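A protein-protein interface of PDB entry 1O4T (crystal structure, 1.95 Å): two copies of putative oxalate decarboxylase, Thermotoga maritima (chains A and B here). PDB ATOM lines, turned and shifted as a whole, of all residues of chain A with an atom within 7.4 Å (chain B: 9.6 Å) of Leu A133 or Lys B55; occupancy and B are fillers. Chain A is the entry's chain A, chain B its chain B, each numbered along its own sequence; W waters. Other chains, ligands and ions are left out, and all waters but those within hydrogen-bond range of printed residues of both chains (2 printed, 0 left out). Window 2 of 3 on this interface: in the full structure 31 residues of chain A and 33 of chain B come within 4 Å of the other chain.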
ATOM      1  N   LYS A  55      15.237   3.554 -23.768  1.00  0.00           N
ATOM      2  CA  LYS A  55      14.664   2.687 -24.802  1.00  0.00           C
ATOM      3  C   LYS A  55      14.051   1.420 -24.208  1.00  0.00           C
ATOM      4  O   LYS A  55      13.194   0.787 -24.825  1.00  0.00           O
ATOM      5  CB  LYS A  55      15.736   2.324 -25.820  1.00  0.00           C
ATOM      6  CG  LYS A  55      16.242   3.519 -26.608  1.00  0.00           C
ATOM      7  CD  LYS A  55      15.138   4.041 -27.522  1.00  0.00           C
ATOM      8  CE  LYS A  55      15.634   5.109 -28.448  1.00  0.00           C
ATOM      9  NZ  LYS A  55      14.487   5.739 -29.174  1.00  0.00           N
ATOM     10  N   GLU A  76       1.189  -2.071 -21.841  1.00  0.00           N
ATOM     11  CA  GLU A  76       0.700  -1.245 -22.940  1.00  0.00           C
ATOM     12  C   GLU A  76       1.745  -0.218 -23.276  1.00  0.00           C
ATOM     13  O   GLU A  76       2.301   0.420 -22.381  1.00  0.00           O
ATOM     14  CB  GLU A  76      -0.657  -0.555 -22.625  1.00  0.00           C
ATOM     15  CG  GLU A  76      -0.843  -0.180 -21.167  1.00  0.00           C
ATOM     16  CD  GLU A  76      -2.262   0.215 -20.802  1.00  0.00           C
ATOM     17  OE1 GLU A  76      -3.017   0.791 -21.647  1.00  0.00           O
ATOM     18  OE2 GLU A  76      -2.611  -0.054 -19.623  1.00  0.00           O
ATOM     19  N   GLY A  77       2.021  -0.081 -24.569  1.00  0.00           N
ATOM     20  CA  GLY A  77       3.019   0.837 -25.037  1.00  0.00           C
ATOM     21  C   GLY A  77       4.438   0.332 -24.828  1.00  0.00           C
ATOM     22  O   GLY A  77       5.386   1.115 -24.894  1.00  0.00           O
ATOM     23  N   GLU A  78       4.578  -0.965 -24.594  1.00  0.00           N
ATOM     24  CA  GLU A  78       5.873  -1.613 -24.400  1.00  0.00           C
ATOM     25  C   GLU A  78       5.699  -3.106 -24.633  1.00  0.00           C
ATOM     26  O   GLU A  78       4.577  -3.580 -24.780  1.00  0.00           O
ATOM     27  CB  GLU A  78       6.400  -1.375 -22.976  1.00  0.00           C
ATOM     28  CG  GLU A  78       5.521  -1.976 -21.902  1.00  0.00           C
ATOM     29  CD  GLU A  78       5.709  -1.382 -20.519  1.00  0.00           C
ATOM     30  OE1 GLU A  78       6.404  -0.349 -20.397  1.00  0.00           O
ATOM     31  OE2 GLU A  78       5.130  -1.971 -19.564  1.00  0.00           O
ATOM     32  N   PHE A  79       6.807  -3.843 -24.656  1.00  0.00           N
ATOM     33  CA  PHE A  79       6.735  -5.284 -24.713  1.00  0.00           C
ATOM     34  C   PHE A  79       7.773  -5.882 -23.786  1.00  0.00           C
ATOM     35  O   PHE A  79       8.750  -5.220 -23.446  1.00  0.00           O
ATOM     36  CB  PHE A  79       6.824  -5.808 -26.157  1.00  0.00           C
ATOM     37  CG  PHE A  79       8.135  -5.534 -26.843  1.00  0.00           C
ATOM     38  CD1 PHE A  79       8.301  -4.402 -27.604  1.00  0.00           C
ATOM     39  CD2 PHE A  79       9.196  -6.428 -26.740  1.00  0.00           C
ATOM     40  CE1 PHE A  79       9.482  -4.150 -28.244  1.00  0.00           C
ATOM     41  CE2 PHE A  79      10.418  -6.151 -27.372  1.00  0.00           C
ATOM     42  CZ  PHE A  79      10.537  -5.000 -28.142  1.00  0.00           C
ATOM     43  N   ASP A 109       3.569  -9.134 -25.914  1.00  0.00           N
ATOM     44  CA  ASP A 109       3.503  -7.992 -26.801  1.00  0.00           C
ATOM     45  C   ASP A 109       2.663  -6.898 -26.172  1.00  0.00           C
ATOM     46  O   ASP A 109       1.965  -7.124 -25.169  1.00  0.00           O
ATOM     47  CB  ASP A 109       2.897  -8.414 -28.148  1.00  0.00           C
ATOM     48  CG  ASP A 109       3.472  -7.644 -29.322  1.00  0.00           C
ATOM     49  OD1 ASP A 109       4.048  -6.541 -29.139  1.00  0.00           O
ATOM     50  OD2 ASP A 109       3.392  -8.088 -30.476  1.00  0.00           O
ATOM     51  N   SER A 110       2.695  -5.716 -26.785  1.00  0.00           N
ATOM     52  CA  SER A 110       1.920  -4.571 -26.292  1.00  0.00           C
ATOM     53  C   SER A 110       0.452  -4.966 -26.308  1.00  0.00           C
ATOM     54  O   SER A 110      -0.020  -5.533 -27.271  1.00  0.00           O
ATOM     55  CB  SER A 110       2.205  -3.348 -27.190  1.00  0.00           C
ATOM     56  OG  SER A 110       1.551  -2.139 -26.757  1.00  0.00           O
ATOM     57  N   ILE A 130      12.002  -5.074 -20.511  1.00  0.00           N
ATOM     58  CA  ILE A 130      10.829  -4.383 -21.024  1.00  0.00           C
ATOM     59  C   ILE A 130      11.324  -3.328 -21.996  1.00  0.00           C
ATOM     60  O   ILE A 130      12.125  -2.507 -21.610  1.00  0.00           O
ATOM     61  CB  ILE A 130      10.013  -3.764 -19.879  1.00  0.00           C
ATOM     62  CG1 ILE A 130       9.529  -4.864 -18.933  1.00  0.00           C
ATOM     63  CG2 ILE A 130       8.806  -2.996 -20.438  1.00  0.00           C
ATOM     64  CD1 ILE A 130       8.857  -4.334 -17.625  1.00  0.00           C
ATOM     65  N   ILE A 131      10.835  -3.358 -23.235  1.00  0.00           N
ATOM     66  CA  ILE A 131      11.278  -2.449 -24.266  1.00  0.00           C
ATOM     67  C   ILE A 131      10.090  -1.575 -24.673  1.00  0.00           C
ATOM     68  O   ILE A 131       8.975  -2.067 -24.950  1.00  0.00           O
ATOM     69  CB  ILE A 131      11.890  -3.254 -25.439  1.00  0.00           C
ATOM     70  CG1 ILE A 131      13.160  -3.996 -24.949  1.00  0.00           C
ATOM     71  CG2 ILE A 131      12.211  -2.371 -26.593  1.00  0.00           C
ATOM     72  CD1 ILE A 131      13.945  -4.755 -26.010  1.00  0.00           C
ATOM     73  N   LEU A 132      10.358  -0.276 -24.697  1.00  0.00           N
ATOM     74  CA  LEU A 132       9.340   0.725 -24.893  1.00  0.00           C
ATOM     75  C   LEU A 132       8.847   0.848 -26.341  1.00  0.00           C
ATOM     76  O   LEU A 132       9.639   0.821 -27.283  1.00  0.00           O
ATOM     77  CB  LEU A 132       9.827   2.075 -24.361  1.00  0.00           C
ATOM     78  CG  LEU A 132      10.194   2.051 -22.866  1.00  0.00           C
ATOM     79  CD1 LEU A 132      10.568   3.446 -22.383  1.00  0.00           C
ATOM     80  CD2 LEU A 132       9.067   1.473 -22.001  1.00  0.00           C
ATOM     81  N   LEU A 133       7.514   0.980 -26.438  1.00  0.00           N
ATOM     82  CA  LEU A 133       6.657   1.115 -27.646  1.00  0.00           C
ATOM     83  C   LEU A 133       6.428  -0.153 -28.493  1.00  0.00           C
ATOM     84  O   LEU A 133       5.300  -0.693 -28.488  1.00  0.00           O
ATOM     85  CB  LEU A 133       7.081   2.301 -28.480  1.00  0.00           C
ATOM     86  CG  LEU A 133       7.254   3.587 -27.662  1.00  0.00           C
ATOM     87  CD1 LEU A 133       7.128   4.717 -28.590  1.00  0.00           C
ATOM     88  CD2 LEU A 133       6.289   3.762 -26.498  1.00  0.00           C
ATOM     89  OXT LEU A 133       7.324  -0.680 -29.180  1.00  0.00           O
ATOM     90  N   SER B  48      13.023 -12.032 -33.961  1.00  0.00           N
ATOM     91  CA  SER B  48      13.367 -11.167 -35.092  1.00  0.00           C
ATOM     92  C   SER B  48      13.202  -9.694 -34.718  1.00  0.00           C
ATOM     93  O   SER B  48      12.490  -9.361 -33.758  1.00  0.00           O
ATOM     94  CB  SER B  48      12.493 -11.492 -36.300  1.00  0.00           C
ATOM     95  OG  SER B  48      11.127 -11.213 -36.030  1.00  0.00           O
ATOM     96  N   LYS B  49      13.879  -8.819 -35.474  1.00  0.00           N
ATOM     97  CA  LYS B  49      13.672  -7.363 -35.373  1.00  0.00           C
ATOM     98  C   LYS B  49      12.206  -6.979 -35.496  1.00  0.00           C
ATOM     99  O   LYS B  49      11.717  -6.159 -34.727  1.00  0.00           O
ATOM    100  CB  LYS B  49      14.473  -6.654 -36.451  1.00  0.00           C
ATOM    101  CG  LYS B  49      14.351  -5.154 -36.500  1.00  0.00           C
ATOM    102  CD  LYS B  49      15.365  -4.575 -37.489  1.00  0.00           C
ATOM    103  CE  LYS B  49      15.238  -3.071 -37.626  1.00  0.00           C
ATOM    104  NZ  LYS B  49      16.015  -2.564 -38.797  1.00  0.00           N
ATOM    105  N   GLU B  50      11.513  -7.583 -36.457  1.00  0.00           N
ATOM    106  CA  GLU B  50      10.107  -7.309 -36.687  1.00  0.00           C
ATOM    107  C   GLU B  50       9.275  -7.513 -35.424  1.00  0.00           C
ATOM    108  O   GLU B  50       8.479  -6.641 -35.047  1.00  0.00           O
ATOM    109  CB  GLU B  50       9.518  -8.204 -37.803  1.00  0.00           C
ATOM    110  CG  GLU B  50       9.396  -7.518 -39.159  1.00  0.00           C
ATOM    111  CD  GLU B  50       8.486  -8.250 -40.162  1.00  0.00           C
ATOM    112  OE1 GLU B  50       7.234  -8.400 -39.910  1.00  0.00           O
ATOM    113  OE2 GLU B  50       9.021  -8.630 -41.248  1.00  0.00           O
ATOM    114  N   ALA B  51       9.446  -8.686 -34.804  1.00  0.00           N
ATOM    115  CA  ALA B  51       8.681  -9.076 -33.616  1.00  0.00           C
ATOM    116  C   ALA B  51       8.931  -8.115 -32.474  1.00  0.00           C
ATOM    117  O   ALA B  51       8.089  -7.932 -31.614  1.00  0.00           O
ATOM    118  CB  ALA B  51       9.073 -10.492 -33.184  1.00  0.00           C
ATOM    119  N   MET B  52      10.117  -7.521 -32.478  1.00  0.00           N
ATOM    120  CA  MET B  52      10.519  -6.561 -31.481  1.00  0.00           C
ATOM    121  C   MET B  52      10.275  -5.135 -31.978  1.00  0.00           C
ATOM    122  O   MET B  52      10.908  -4.202 -31.509  1.00  0.00           O
ATOM    123  CB  MET B  52      12.002  -6.784 -31.135  1.00  0.00           C
ATOM    124  CG  MET B  52      12.331  -8.187 -30.574  1.00  0.00           C
ATOM    125  SD  MET B  52      14.024  -8.331 -29.987  1.00  0.00           S
ATOM    126  CE  MET B  52      14.970  -8.489 -31.529  1.00  0.00           C
ATOM    127  N   HIS B  53       9.365  -4.984 -32.936  1.00  0.00           N
ATOM    128  CA  HIS B  53       8.831  -3.676 -33.376  1.00  0.00           C
ATOM    129  C   HIS B  53       9.925  -2.760 -33.908  1.00  0.00           C
ATOM    130  O   HIS B  53       9.808  -1.547 -33.817  1.00  0.00           O
ATOM    131  CB  HIS B  53       8.071  -2.978 -32.233  1.00  0.00           C
ATOM    132  CG  HIS B  53       6.867  -3.731 -31.749  1.00  0.00           C
ATOM    133  ND1 HIS B  53       5.581  -3.366 -32.079  1.00  0.00           N
ATOM    134  CD2 HIS B  53       6.750  -4.815 -30.959  1.00  0.00           C
ATOM    135  CE1 HIS B  53       4.727  -4.187 -31.496  1.00  0.00           C
ATOM    136  NE2 HIS B  53       5.413  -5.088 -30.824  1.00  0.00           N
ATOM    137  N   ASN B  54      11.001  -3.347 -34.436  1.00  0.00           N
ATOM    138  CA  ASN B  54      12.129  -2.587 -34.940  1.00  0.00           C
ATOM    139  C   ASN B  54      12.847  -1.755 -33.874  1.00  0.00           C
ATOM    140  O   ASN B  54      13.496  -0.766 -34.223  1.00  0.00           O
ATOM    141  CB  ASN B  54      11.680  -1.671 -36.089  1.00  0.00           C
ATOM    142  CG  ASN B  54      11.078  -2.435 -37.269  1.00  0.00           C
ATOM    143  OD1 ASN B  54      11.651  -3.405 -37.758  1.00  0.00           O
ATOM    144  ND2 ASN B  54       9.960  -1.939 -37.784  1.00  0.00           N
ATOM    145  N   LYS B  55      12.719  -2.135 -32.595  1.00  0.00           N
ATOM    146  CA  LYS B  55      13.363  -1.433 -31.470  1.00  0.00           C
ATOM    147  C   LYS B  55      14.704  -2.100 -31.124  1.00  0.00           C
ATOM    148  O   LYS B  55      15.575  -1.487 -30.506  1.00  0.00           O
ATOM    149  CB  LYS B  55      12.458  -1.441 -30.215  1.00  0.00           C
ATOM    150  CG  LYS B  55      11.164  -0.609 -30.317  1.00  0.00           C
ATOM    151  CD  LYS B  55      11.503   0.825 -30.703  1.00  0.00           C
ATOM    152  CE  LYS B  55      10.372   1.764 -30.488  1.00  0.00           C
ATOM    153  NZ  LYS B  55      10.834   3.145 -30.810  1.00  0.00           N
ATOM    154  N   ALA B  56      14.819  -3.386 -31.451  1.00  0.00           N
ATOM    155  CA  ALA B  56      16.060  -4.126 -31.280  1.00  0.00           C
ATOM    156  C   ALA B  56      16.291  -4.869 -32.579  1.00  0.00           C
ATOM    157  O   ALA B  56      15.318  -5.216 -33.270  1.00  0.00           O
ATOM    158  CB  ALA B  56      15.970  -5.081 -30.115  1.00  0.00           C
ATOM    159  N   ARG B  57      17.560  -5.030 -32.955  1.00  0.00           N
ATOM    160  CA  ARG B  57      17.900  -5.693 -34.211  1.00  0.00           C
ATOM    161  C   ARG B  57      18.471  -7.109 -34.029  1.00  0.00           C
ATOM    162  O   ARG B  57      18.643  -7.847 -34.993  1.00  0.00           O
ATOM    163  CB  ARG B  57      18.788  -4.802 -35.091  1.00  0.00           C
ATOM    164  CG  ARG B  57      20.238  -4.654 -34.750  1.00  0.00           C
ATOM    165  CD  ARG B  57      20.995  -3.946 -35.849  1.00  0.00           C
ATOM    166  NE  ARG B  57      22.432  -3.836 -35.577  1.00  0.00           N
ATOM    167  CZ  ARG B  57      23.308  -4.818 -35.735  1.00  0.00           C
ATOM    168  NH1 ARG B  57      22.940  -5.993 -36.205  1.00  0.00           N
ATOM    169  NH2 ARG B  57      24.579  -4.623 -35.447  1.00  0.00           N
ATOM    170  N   LEU B  58      18.712  -7.496 -32.792  1.00  0.00           N
ATOM    171  CA  LEU B  58      19.242  -8.825 -32.501  1.00  0.00           C
ATOM    172  C   LEU B  58      18.823  -9.246 -31.115  1.00  0.00           C
ATOM    173  O   LEU B  58      18.893  -8.448 -30.187  1.00  0.00           O
ATOM    174  CB  LEU B  58      20.768  -8.812 -32.594  1.00  0.00           C
ATOM    175  CG  LEU B  58      21.540 -10.134 -32.396  1.00  0.00           C
ATOM    176  CD1 LEU B  58      21.305 -11.027 -33.602  1.00  0.00           C
ATOM    177  CD2 LEU B  58      23.032  -9.917 -32.198  1.00  0.00           C
ATOM    178  N   PHE B  59      18.366 -10.491 -31.002  1.00  0.00           N
ATOM    179  CA  PHE B  59      18.192 -11.188 -29.718  1.00  0.00           C
ATOM    180  C   PHE B  59      18.614 -12.641 -29.912  1.00  0.00           C
ATOM    181  O   PHE B  59      17.825 -13.500 -30.375  1.00  0.00           O
ATOM    182  CB  PHE B  59      16.731 -11.123 -29.218  1.00  0.00           C
ATOM    183  CG  PHE B  59      16.564 -11.491 -27.765  1.00  0.00           C
ATOM    184  CD1 PHE B  59      16.181 -12.742 -27.397  1.00  0.00           C
ATOM    185  CD2 PHE B  59      16.828 -10.572 -26.756  1.00  0.00           C
ATOM    186  CE1 PHE B  59      16.063 -13.099 -26.067  1.00  0.00           C
ATOM    187  CE2 PHE B  59      16.707 -10.931 -25.414  1.00  0.00           C
ATOM    188  CZ  PHE B  59      16.334 -12.216 -25.086  1.00  0.00           C
ATOM    189  N   GLY B  77      25.001   4.239 -33.299  1.00  0.00           N
ATOM    190  CA  GLY B  77      23.540   4.375 -33.383  1.00  0.00           C
ATOM    191  C   GLY B  77      22.739   3.279 -32.674  1.00  0.00           C
ATOM    192  O   GLY B  77      21.551   3.109 -32.937  1.00  0.00           O
ATOM    193  N   GLU B  78      23.399   2.539 -31.778  1.00  0.00           N
ATOM    194  CA  GLU B  78      22.769   1.462 -31.037  1.00  0.00           C
ATOM    195  C   GLU B  78      23.674   1.097 -29.882  1.00  0.00           C
ATOM    196  O   GLU B  78      24.800   1.560 -29.805  1.00  0.00           O
ATOM    197  CB  GLU B  78      22.598   0.244 -31.931  1.00  0.00           C
ATOM    198  CG  GLU B  78      23.944  -0.311 -32.392  1.00  0.00           C
ATOM    199  CD  GLU B  78      23.861  -1.226 -33.607  1.00  0.00           C
ATOM    200  OE1 GLU B  78      22.787  -1.287 -34.256  1.00  0.00           O
ATOM    201  OE2 GLU B  78      24.885  -1.907 -33.891  1.00  0.00           O
ATOM    202  N   PHE B  79      23.176   0.260 -28.981  1.00  0.00           N
ATOM    203  CA  PHE B  79      23.987  -0.313 -27.918  1.00  0.00           C
ATOM    204  C   PHE B  79      23.674  -1.787 -27.822  1.00  0.00           C
ATOM    205  O   PHE B  79      22.670  -2.243 -28.374  1.00  0.00           O
ATOM    206  CB  PHE B  79      23.787   0.412 -26.578  1.00  0.00           C
ATOM    207  CG  PHE B  79      22.380   0.355 -26.033  1.00  0.00           C
ATOM    208  CD1 PHE B  79      21.436   1.301 -26.412  1.00  0.00           C
ATOM    209  CD2 PHE B  79      22.009  -0.639 -25.104  1.00  0.00           C
ATOM    210  CE1 PHE B  79      20.163   1.263 -25.892  1.00  0.00           C
ATOM    211  CE2 PHE B  79      20.719  -0.691 -24.590  1.00  0.00           C
ATOM    212  CZ  PHE B  79      19.802   0.262 -24.985  1.00  0.00           C
ATOM    213  N   VAL B 129      21.891  -8.767 -27.113  1.00  0.00           N
ATOM    214  CA  VAL B 129      20.775  -7.962 -27.574  1.00  0.00           C
ATOM    215  C   VAL B 129      21.258  -6.618 -27.990  1.00  0.00           C
ATOM    216  O   VAL B 129      21.961  -5.941 -27.236  1.00  0.00           O
ATOM    217  CB  VAL B 129      19.633  -7.865 -26.478  1.00  0.00           C
ATOM    218  CG1 VAL B 129      20.067  -7.181 -25.275  1.00  0.00           C
ATOM    219  CG2 VAL B 129      18.438  -7.188 -26.994  1.00  0.00           C
ATOM    220  N   ILE B 130      20.880  -6.215 -29.207  1.00  0.00           N
ATOM    221  CA  ILE B 130      21.262  -4.928 -29.747  1.00  0.00           C
ATOM    222  C   ILE B 130      20.068  -4.011 -29.886  1.00  0.00           C
ATOM    223  O   ILE B 130      19.179  -4.257 -30.686  1.00  0.00           O
ATOM    224  CB  ILE B 130      21.953  -5.072 -31.112  1.00  0.00           C
ATOM    225  CG1 ILE B 130      23.176  -5.984 -31.001  1.00  0.00           C
ATOM    226  CG2 ILE B 130      22.339  -3.664 -31.649  1.00  0.00           C
ATOM    227  CD1 ILE B 130      23.827  -6.265 -32.360  1.00  0.00           C
ATOM    228  N   ILE B 131      20.081  -2.932 -29.121  1.00  0.00           N
ATOM    229  CA  ILE B 131      18.948  -2.032 -29.076  1.00  0.00           C
ATOM    230  C   ILE B 131      19.305  -0.736 -29.777  1.00  0.00           C
ATOM    231  O   ILE B 131      20.372  -0.141 -29.555  1.00  0.00           O
ATOM    232  CB  ILE B 131      18.538  -1.792 -27.635  1.00  0.00           C
ATOM    233  CG1 ILE B 131      18.039  -3.094 -27.029  1.00  0.00           C
ATOM    234  CG2 ILE B 131      17.451  -0.709 -27.569  1.00  0.00           C
ATOM    235  CD1 ILE B 131      17.792  -3.006 -25.555  1.00  0.00           C
ATOM    236  N   LEU B 132      18.374  -0.292 -30.607  1.00  0.00           N
ATOM    237  CA  LEU B 132      18.644   0.765 -31.560  1.00  0.00           C
ATOM    238  C   LEU B 132      18.527   2.154 -30.939  1.00  0.00           C
ATOM    239  O   LEU B 132      17.632   2.403 -30.117  1.00  0.00           O
ATOM    240  CB  LEU B 132      17.728   0.619 -32.780  1.00  0.00           C
ATOM    241  CG  LEU B 132      17.849  -0.734 -33.478  1.00  0.00           C
ATOM    242  CD1 LEU B 132      16.917  -0.774 -34.636  1.00  0.00           C
ATOM    243  CD2 LEU B 132      19.288  -0.997 -33.939  1.00  0.00           C
ATOM    244  N   LEU B 133      19.477   3.006 -31.353  1.00  0.00           N
ATOM    245  CA  LEU B 133      19.695   4.409 -30.912  1.00  0.00           C
ATOM    246  C   LEU B 133      20.225   4.612 -29.466  1.00  0.00           C
ATOM    247  O   LEU B 133      21.446   4.870 -29.286  1.00  0.00           O
ATOM    248  CB  LEU B 133      18.476   5.275 -31.215  1.00  0.00           C
ATOM    249  CG  LEU B 133      18.238   5.635 -32.687  1.00  0.00           C
ATOM    250  CD1 LEU B 133      18.711   7.087 -33.019  1.00  0.00           C
ATOM    251  CD2 LEU B 133      18.828   4.619 -33.684  1.00  0.00           C
ATOM    252  OXT LEU B 133      19.483   4.527 -28.463  1.00  0.00           O
HETATM  253  O   HOH W   1       5.560  -8.081 -32.439  1.00  0.00           O
HETATM  254  O   HOH W   2      14.141   3.296 -30.926  1.00  0.00           O
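Water W1 lies within hydrogen-bond range of the backbone carbonyl oxygen of Ala B51 (2.7 Å), the side-chain carboxylate of Asp A109 (2.9 Å) and a ring nitrogen (NE2) of His B53 (3.4 Å).
Water W2 bridges NZ of Lys A55 and NZ of Lys B55.
Of the printed residues of chain B, Lys A55 touches Ile B131, Leu B132 and Leu B133.
Printed residues of chain A within 4 Å of Met B52: Phe A79.
Printed residues of chain A within 4 Å of His B53: Phe A79 (3.7 Å), Asp A109 (2.6 Å) and Leu A133 (3.9 Å).
Arg B57 touches none of the printed residues of chain A.
Of the printed residues of chain A, Ile B131 touches Lys A55 (3.9 Å).
Printed residues of chain A within 4 Å of Leu B132: Lys A55.
The nearest residue of chain B that does not touch Leu A133 is Met B52 (5.5 Å).
Hydrophobic or aromatic side chains of chain B that line the printed part of chain A: Met B52, His B53, Ile B131 and Leu B133.
Of the 11 printed residues of chain A, 6 touch a printed residue of chain B.
O of Lys A55 is in hydrogen-bond range of N of Leu A132 (3.0 Å).
O of Gly A77 is in hydrogen-bond range of N of Leu A133, at 2.6 Å.
O of Phe A79 sits at hydrogen-bond distance from N of Ile A131.
The backbone NH (N) of Leu B132 lies within hydrogen-bond range of the backbone carbonyl oxygen (O) of Lys B55, 3.0 Å away.
O of Gly B77 is in hydrogen-bond range of N of Leu B133, at 2.6 Å.
The backbone carbonyl oxygen (O) of Phe B79 sits at hydrogen-bond distance from the backbone NH (N) of Ile B131.
Lys A55 touches Ile B131 (CB to CG2, 3.9 Å).
Lys A55 touches Leu B132.
Leu B133 touches Lys A55.
Met B52 touches Phe A79 (O to CZ, 3.5 Å).
CD2 of His B53 touches CD1 of Phe A79, 3.7 Å away.
CG2 of Ile A131 touches CB of Lys B55, at 3.7 Å.
Leu A132 touches Lys B55.
OXT of Leu A133 touches CB of His B53 (3.9 Å).
Leu A133 touches Lys B55.
Lys A55 touches Ile B131, and with the chains exchanged Ile A131 touches Lys B55.
Lys A55 touches Leu B132, and with the chains exchanged Leu A132 touches Lys B55.
Lys A55 touches Leu B133, and with the chains exchanged Leu A133 touches Lys B55.
8 positions are printed for both chains.
Of the 10 pairs that touch across the chains among the printed residues, 6 have their exchanged pair printed and touching as well.
OD1 of Asp A109 lies within hydrogen-bond range of NE2 of His B53.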
